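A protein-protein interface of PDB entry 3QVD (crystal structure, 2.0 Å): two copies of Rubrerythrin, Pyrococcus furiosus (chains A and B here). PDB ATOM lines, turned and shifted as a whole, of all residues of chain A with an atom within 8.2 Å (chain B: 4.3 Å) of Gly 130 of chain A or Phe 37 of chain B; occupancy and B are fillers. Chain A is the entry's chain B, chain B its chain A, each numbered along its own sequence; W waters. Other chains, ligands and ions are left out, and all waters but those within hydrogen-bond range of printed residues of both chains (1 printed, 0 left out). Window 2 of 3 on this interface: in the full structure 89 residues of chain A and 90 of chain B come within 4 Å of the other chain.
The backbone NH of Asn 39 of chain B sits at hydrogen-bond distance from the side-chain carboxylate of Asp 132 of chain A (2.8 Å). The side-chain amide nitrogen of Asn 39 of chain B sits at hydrogen-bond distance from the backbone carbonyl oxygen of Ile 133 of chain A. OD2 of Asp 132 of chain A lies within hydrogen-bond range of N of Ile 40 of chain B (3.1 Å). The side-chain carboxylate (OE2) of Glu 35 of chain B lies within hydrogen-bond range of the side-chain hydroxyl (OG1) of Thr 68 of chain A. OD1 of Asp 132 of chain A sits close to N of Pro 38 of chain B (3.4 Å).
N of Phe 37 of chain B sits at hydrogen-bond distance from O of Ala 32 of chain B, 2.9 Å away. OE2 of Glu 131 of chain A is in salt-bridge range of NZ of Lys 129 of chain A (3.3 Å). NZ of Lys 126 of chain A is in salt-bridge range of OE1 of Glu 131 of chain A (2.7 Å).
Among the printed residues, merely in contact across the chains: Lys 67 of chain A with Glu 35 of chain B (3.2 Å), Thr 68 of chain A with Ala 32 of chain B (3.3 Å), Thr 68 of chain A with Phe 37 of chain B (3.5 Å), Thr 68 of chain A with Ile 40 of chain B (3.9 Å), Ala 127 of chain A with Ile 40 of chain B (3.9 Å), Gly 130 of chain A with Phe 37 of chain B (3.8 Å), Glu 131 of chain A with Phe 37 of chain B (3.8 Å), Asp 132 of chain A with Phe 37 of chain B (3.7 Å) and Ile 133 of chain A with Ile 40 of chain B (3.7 Å).
Of the printed residues of chain B, Ala 127 of chain A touches Ile 40 (3.9 Å). Lys 129 of chain A touches none of the printed residues of chain B. Of chain B, only Phe 37 comes within 4 Å of Gly 130 of chain A. Printed residues of chain B within 4 Å of Asp 132 of chain A: Phe 37 (3.7 Å), Pro 38 (3.3 Å), Asn 39 (2.8 Å) and Ile 40 (3.1 Å). No residue of chain A comes within 4 Å of Gly 36 of chain B. Phe 37 of chain B touches just these residues of chain A: Thr 68, Gly 130, Glu 131 and Asp 132. Of the printed residues of chain A, Asn 39 of chain B touches Asp 132 (2.8 Å) and Ile 133 (2.8 Å). Ala 41 of chain B touches none of the printed residues of chain A.
Of the 15 printed residues of chain A, 7 touch a printed residue of chain B. Hydrophobic or aromatic side chains of chain A within 4 Å of the printed part of chain B: Ala 127 and Ile 133. Of the 8 printed residues of chain B, 6 touch a printed residue of chain A. Hydrophobic or aromatic side chains of chain B within 4 Å of the printed part of chain A: Ala 32, Phe 37, Pro 38 and Ile 40. Among the printed residues, 14 pairs touch across the chains.
No position is printed for both chains.
Water W1 bridges the side-chain hydroxyl (OG1) of Thr 68 of chain A (3.0 Å) and the backbone NH (N) of Ala 32 of chain B (3.4 Å).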
ATOM      1  N   LYS A  67     -14.014  -1.934  -7.257  1.00  0.00           N
ATOM      2  CA  LYS A  67     -12.709  -1.772  -7.896  1.00  0.00           C
ATOM      3  C   LYS A  67     -12.918  -1.930  -9.399  1.00  0.00           C
ATOM      4  O   LYS A  67     -13.931  -2.475  -9.833  1.00  0.00           O
ATOM      5  CB  LYS A  67     -11.716  -2.827  -7.394  1.00  0.00           C
ATOM      6  CG  LYS A  67     -11.429  -2.770  -5.901  1.00  0.00           C
ATOM      7  CD  LYS A  67     -10.217  -3.635  -5.552  1.00  0.00           C
ATOM      8  CE  LYS A  67     -10.005  -3.734  -4.053  1.00  0.00           C
ATOM      9  NZ  LYS A  67     -11.085  -4.523  -3.399  1.00  0.00           N
ATOM     10  N   THR A  68     -11.957  -1.463 -10.187  1.00  0.00           N
ATOM     11  CA  THR A  68     -12.052  -1.520 -11.644  1.00  0.00           C
ATOM     12  C   THR A  68     -12.484  -2.860 -12.248  1.00  0.00           C
ATOM     13  O   THR A  68     -13.335  -2.892 -13.137  1.00  0.00           O
ATOM     14  CB  THR A  68     -10.724  -1.080 -12.292  1.00  0.00           C
ATOM     15  OG1 THR A  68     -10.481   0.296 -11.975  1.00  0.00           O
ATOM     16  CG2 THR A  68     -10.781  -1.240 -13.804  1.00  0.00           C
ATOM     17  N   PRO A  69     -11.902  -3.983 -11.787  1.00  0.00           N
ATOM     18  CA  PRO A  69     -12.299  -5.276 -12.350  1.00  0.00           C
ATOM     19  C   PRO A  69     -13.798  -5.530 -12.200  1.00  0.00           C
ATOM     20  O   PRO A  69     -14.456  -5.983 -13.140  1.00  0.00           O
ATOM     21  CB  PRO A  69     -11.459  -6.273 -11.551  1.00  0.00           C
ATOM     22  CG  PRO A  69     -10.222  -5.491 -11.244  1.00  0.00           C
ATOM     23  CD  PRO A  69     -10.795  -4.153 -10.828  1.00  0.00           C
ATOM     24  N   LEU A  72     -15.836  -3.204 -14.441  1.00  0.00           N
ATOM     25  CA  LEU A  72     -15.815  -3.670 -15.824  1.00  0.00           C
ATOM     26  C   LEU A  72     -16.836  -4.796 -15.989  1.00  0.00           C
ATOM     27  O   LEU A  72     -17.491  -4.918 -17.027  1.00  0.00           O
ATOM     28  CB  LEU A  72     -14.412  -4.168 -16.197  1.00  0.00           C
ATOM     29  CG  LEU A  72     -13.366  -3.087 -16.484  1.00  0.00           C
ATOM     30  CD1 LEU A  72     -11.971  -3.699 -16.508  1.00  0.00           C
ATOM     31  CD2 LEU A  72     -13.683  -2.412 -17.818  1.00  0.00           C
ATOM     32  N   ALA A 123     -10.307  -5.671 -21.389  1.00  0.00           N
ATOM     33  CA  ALA A 123      -9.795  -4.823 -20.318  1.00  0.00           C
ATOM     34  C   ALA A 123      -9.808  -5.499 -18.952  1.00  0.00           C
ATOM     35  O   ALA A 123      -8.871  -5.335 -18.170  1.00  0.00           O
ATOM     36  CB  ALA A 123     -10.590  -3.510 -20.260  1.00  0.00           C
ATOM     37  N   LYS A 124     -10.861  -6.256 -18.660  1.00  0.00           N
ATOM     38  CA  LYS A 124     -10.959  -6.926 -17.369  1.00  0.00           C
ATOM     39  C   LYS A 124      -9.876  -7.986 -17.161  1.00  0.00           C
ATOM     40  O   LYS A 124      -9.342  -8.129 -16.060  1.00  0.00           O
ATOM     41  CB  LYS A 124     -12.337  -7.575 -17.197  1.00  0.00           C
ATOM     42  CG  LYS A 124     -12.531  -8.197 -15.818  1.00  0.00           C
ATOM     43  CD  LYS A 124     -13.859  -8.922 -15.674  1.00  0.00           C
ATOM     44  CE  LYS A 124     -13.998  -9.497 -14.272  1.00  0.00           C
ATOM     45  NZ  LYS A 124     -15.247 -10.285 -14.079  1.00  0.00           N
ATOM     46  N   GLU A 125      -9.561  -8.733 -18.214  1.00  0.00           N
ATOM     47  CA  GLU A 125      -8.540  -9.776 -18.129  1.00  0.00           C
ATOM     48  C   GLU A 125      -7.203  -9.163 -17.712  1.00  0.00           C
ATOM     49  O   GLU A 125      -6.399  -9.799 -17.035  1.00  0.00           O
ATOM     50  CB  GLU A 125      -8.411 -10.486 -19.483  1.00  0.00           C
ATOM     51  CG  GLU A 125      -7.475 -11.694 -19.505  1.00  0.00           C
ATOM     52  CD  GLU A 125      -6.011 -11.309 -19.658  1.00  0.00           C
ATOM     53  OE1 GLU A 125      -5.693 -10.555 -20.604  1.00  0.00           O
ATOM     54  OE2 GLU A 125      -5.179 -11.768 -18.844  1.00  0.00           O
ATOM     55  N   LYS A 126      -6.975  -7.920 -18.120  1.00  0.00           N
ATOM     56  CA  LYS A 126      -5.748  -7.216 -17.776  1.00  0.00           C
ATOM     57  C   LYS A 126      -5.835  -6.636 -16.368  1.00  0.00           C
ATOM     58  O   LYS A 126      -4.889  -6.734 -15.585  1.00  0.00           O
ATOM     59  CB  LYS A 126      -5.485  -6.092 -18.780  1.00  0.00           C
ATOM     60  CG  LYS A 126      -4.739  -6.529 -20.031  1.00  0.00           C
ATOM     61  CD  LYS A 126      -3.311  -6.926 -19.687  1.00  0.00           C
ATOM     62  CE  LYS A 126      -2.467  -7.121 -20.930  1.00  0.00           C
ATOM     63  NZ  LYS A 126      -1.049  -7.413 -20.576  1.00  0.00           N
ATOM     64  N   ALA A 127      -6.975  -6.031 -16.051  1.00  0.00           N
ATOM     65  CA  ALA A 127      -7.186  -5.434 -14.739  1.00  0.00           C
ATOM     66  C   ALA A 127      -7.097  -6.484 -13.634  1.00  0.00           C
ATOM     67  O   ALA A 127      -6.591  -6.209 -12.548  1.00  0.00           O
ATOM     68  CB  ALA A 127      -8.544  -4.737 -14.694  1.00  0.00           C
ATOM     69  N   GLU A 128      -7.596  -7.685 -13.917  1.00  0.00           N
ATOM     70  CA  GLU A 128      -7.567  -8.785 -12.953  1.00  0.00           C
ATOM     71  C   GLU A 128      -6.140  -9.114 -12.522  1.00  0.00           C
ATOM     72  O   GLU A 128      -5.908  -9.541 -11.392  1.00  0.00           O
ATOM     73  CB  GLU A 128      -8.208 -10.042 -13.555  1.00  0.00           C
ATOM     74  CG  GLU A 128      -9.709  -9.952 -13.771  1.00  0.00           C
ATOM     75  CD  GLU A 128     -10.498 -10.040 -12.478  1.00  0.00           C
ATOM     76  OE1 GLU A 128     -10.187  -9.277 -11.538  1.00  0.00           O
ATOM     77  OE2 GLU A 128     -11.435 -10.869 -12.407  1.00  0.00           O
ATOM     78  N   LYS A 129      -5.191  -8.918 -13.432  1.00  0.00           N
ATOM     79  CA  LYS A 129      -3.786  -9.202 -13.153  1.00  0.00           C
ATOM     80  C   LYS A 129      -3.048  -7.951 -12.695  1.00  0.00           C
ATOM     81  O   LYS A 129      -1.819  -7.936 -12.638  1.00  0.00           O
ATOM     82  CB  LYS A 129      -3.101  -9.760 -14.403  1.00  0.00           C
ATOM     83  CG  LYS A 129      -3.754 -11.011 -14.978  1.00  0.00           C
ATOM     84  CD  LYS A 129      -3.024 -11.497 -16.227  1.00  0.00           C
ATOM     85  CE  LYS A 129      -3.017 -10.439 -17.323  1.00  0.00           C
ATOM     86  NZ  LYS A 129      -2.277 -10.873 -18.547  1.00  0.00           N
ATOM     87  N   GLY A 130      -3.799  -6.901 -12.376  1.00  0.00           N
ATOM     88  CA  GLY A 130      -3.189  -5.661 -11.929  1.00  0.00           C
ATOM     89  C   GLY A 130      -2.526  -4.875 -13.049  1.00  0.00           C
ATOM     90  O   GLY A 130      -1.747  -3.953 -12.793  1.00  0.00           O
ATOM     91  N   GLU A 131      -2.842  -5.228 -14.291  1.00  0.00           N
ATOM     92  CA  GLU A 131      -2.266  -4.560 -15.454  1.00  0.00           C
ATOM     93  C   GLU A 131      -3.271  -3.659 -16.167  1.00  0.00           C
ATOM     94  O   GLU A 131      -4.463  -3.953 -16.205  1.00  0.00           O
ATOM     95  CB  GLU A 131      -1.756  -5.597 -16.455  1.00  0.00           C
ATOM     96  CG  GLU A 131      -0.728  -6.567 -15.907  1.00  0.00           C
ATOM     97  CD  GLU A 131      -0.440  -7.701 -16.875  1.00  0.00           C
ATOM     98  OE1 GLU A 131      -0.042  -7.418 -18.024  1.00  0.00           O
ATOM     99  OE2 GLU A 131      -0.616  -8.876 -16.484  1.00  0.00           O
ATOM    100  N   ASP A 132      -2.774  -2.566 -16.739  1.00  0.00           N
ATOM    101  CA  ASP A 132      -3.617  -1.638 -17.483  1.00  0.00           C
ATOM    102  C   ASP A 132      -3.697  -2.198 -18.898  1.00  0.00           C
ATOM    103  O   ASP A 132      -2.925  -3.090 -19.257  1.00  0.00           O
ATOM    104  CB  ASP A 132      -2.982  -0.246 -17.520  1.00  0.00           C
ATOM    105  CG  ASP A 132      -3.948   0.826 -18.001  1.00  0.00           C
ATOM    106  OD1 ASP A 132      -3.500   1.973 -18.219  1.00  0.00           O
ATOM    107  OD2 ASP A 132      -5.155   0.524 -18.153  1.00  0.00           O
ATOM    108  N   ILE A 133      -4.627  -1.689 -19.697  1.00  0.00           N
ATOM    109  CA  ILE A 133      -4.771  -2.160 -21.068  1.00  0.00           C
ATOM    110  C   ILE A 133      -3.835  -1.404 -21.996  1.00  0.00           C
ATOM    111  O   ILE A 133      -3.504  -0.245 -21.749  1.00  0.00           O
ATOM    112  CB  ILE A 133      -6.213  -1.983 -21.580  1.00  0.00           C
ATOM    113  CG1 ILE A 133      -6.663  -0.534 -21.382  1.00  0.00           C
ATOM    114  CG2 ILE A 133      -7.133  -2.952 -20.867  1.00  0.00           C
ATOM    115  CD1 ILE A 133      -8.059  -0.253 -21.890  1.00  0.00           C
ATOM    116  N   ALA B  32     -11.133   4.182 -12.076  1.00  0.00           N
ATOM    117  CA  ALA B  32     -10.017   3.504 -12.735  1.00  0.00           C
ATOM    118  C   ALA B  32      -8.772   4.396 -12.712  1.00  0.00           C
ATOM    119  O   ALA B  32      -7.653   3.921 -12.506  1.00  0.00           O
ATOM    120  CB  ALA B  32     -10.386   3.150 -14.178  1.00  0.00           C
ATOM    121  N   GLU B  35      -7.202   4.275  -9.411  1.00  0.00           N
ATOM    122  CA  GLU B  35      -6.589   2.986  -9.119  1.00  0.00           C
ATOM    123  C   GLU B  35      -5.303   2.729  -9.896  1.00  0.00           C
ATOM    124  O   GLU B  35      -4.603   1.753  -9.637  1.00  0.00           O
ATOM    125  CB  GLU B  35      -7.591   1.855  -9.368  1.00  0.00           C
ATOM    126  CG  GLU B  35      -8.630   1.723  -8.265  1.00  0.00           C
ATOM    127  CD  GLU B  35      -9.539   0.521  -8.434  1.00  0.00           C
ATOM    128  OE1 GLU B  35     -10.056   0.030  -7.414  1.00  0.00           O
ATOM    129  OE2 GLU B  35      -9.750   0.070  -9.579  1.00  0.00           O
ATOM    130  N   GLY B  36      -4.995   3.602 -10.847  1.00  0.00           N
ATOM    131  CA  GLY B  36      -3.779   3.436 -11.622  1.00  0.00           C
ATOM    132  C   GLY B  36      -3.960   2.752 -12.963  1.00  0.00           C
ATOM    133  O   GLY B  36      -3.032   2.109 -13.460  1.00  0.00           O
ATOM    134  N   PHE B  37      -5.150   2.879 -13.547  1.00  0.00           N
ATOM    135  CA  PHE B  37      -5.436   2.286 -14.853  1.00  0.00           C
ATOM    136  C   PHE B  37      -5.882   3.406 -15.789  1.00  0.00           C
ATOM    137  O   PHE B  37      -7.051   3.484 -16.167  1.00  0.00           O
ATOM    138  CB  PHE B  37      -6.553   1.238 -14.745  1.00  0.00           C
ATOM    139  CG  PHE B  37      -6.248   0.115 -13.796  1.00  0.00           C
ATOM    140  CD1 PHE B  37      -7.029  -0.083 -12.662  1.00  0.00           C
ATOM    141  CD2 PHE B  37      -5.184  -0.753 -14.037  1.00  0.00           C
ATOM    142  CE1 PHE B  37      -6.760  -1.128 -11.782  1.00  0.00           C
ATOM    143  CE2 PHE B  37      -4.905  -1.803 -13.162  1.00  0.00           C
ATOM    144  CZ  PHE B  37      -5.696  -1.991 -12.033  1.00  0.00           C
ATOM    145  N   PRO B  38      -4.949   4.291 -16.176  1.00  0.00           N
ATOM    146  CA  PRO B  38      -5.272   5.406 -17.070  1.00  0.00           C
ATOM    147  C   PRO B  38      -5.855   5.020 -18.426  1.00  0.00           C
ATOM    148  O   PRO B  38      -6.717   5.727 -18.953  1.00  0.00           O
ATOM    149  CB  PRO B  38      -3.940   6.154 -17.187  1.00  0.00           C
ATOM    150  CG  PRO B  38      -2.914   5.061 -16.994  1.00  0.00           C
ATOM    151  CD  PRO B  38      -3.511   4.274 -15.852  1.00  0.00           C
ATOM    152  N   ASN B  39      -5.397   3.906 -18.994  1.00  0.00           N
ATOM    153  CA  ASN B  39      -5.908   3.482 -20.292  1.00  0.00           C
ATOM    154  C   ASN B  39      -7.320   2.920 -20.181  1.00  0.00           C
ATOM    155  O   ASN B  39      -8.140   3.104 -21.078  1.00  0.00           O
ATOM    156  CB  ASN B  39      -4.968   2.462 -20.940  1.00  0.00           C
ATOM    157  CG  ASN B  39      -3.662   3.087 -21.390  1.00  0.00           C
ATOM    158  OD1 ASN B  39      -3.637   4.235 -21.837  1.00  0.00           O
ATOM    159  ND2 ASN B  39      -2.571   2.332 -21.292  1.00  0.00           N
ATOM    160  N   ILE B  40      -7.603   2.233 -19.080  1.00  0.00           N
ATOM    161  CA  ILE B  40      -8.939   1.691 -18.866  1.00  0.00           C
ATOM    162  C   ILE B  40      -9.883   2.869 -18.611  1.00  0.00           C
ATOM    163  O   ILE B  40     -11.040   2.856 -19.030  1.00  0.00           O
ATOM    164  CB  ILE B  40      -8.969   0.727 -17.662  1.00  0.00           C
ATOM    165  CG1 ILE B  40      -8.204  -0.559 -18.012  1.00  0.00           C
ATOM    166  CG2 ILE B  40     -10.417   0.401 -17.284  1.00  0.00           C
ATOM    167  CD1 ILE B  40      -8.179  -1.598 -16.897  1.00  0.00           C
ATOM    168  N   ALA B  41      -9.374   3.894 -17.931  1.00  0.00           N
ATOM    169  CA  ALA B  41     -10.174   5.080 -17.646  1.00  0.00           C
ATOM    170  C   ALA B  41     -10.506   5.762 -18.964  1.00  0.00           C
ATOM    171  O   ALA B  41     -11.630   6.227 -19.169  1.00  0.00           O
ATOM    172  CB  ALA B  41      -9.405   6.030 -16.740  1.00  0.00           C
HETATM  173  O   HOH W   1     -13.175   1.535 -12.591  1.00  0.00           O
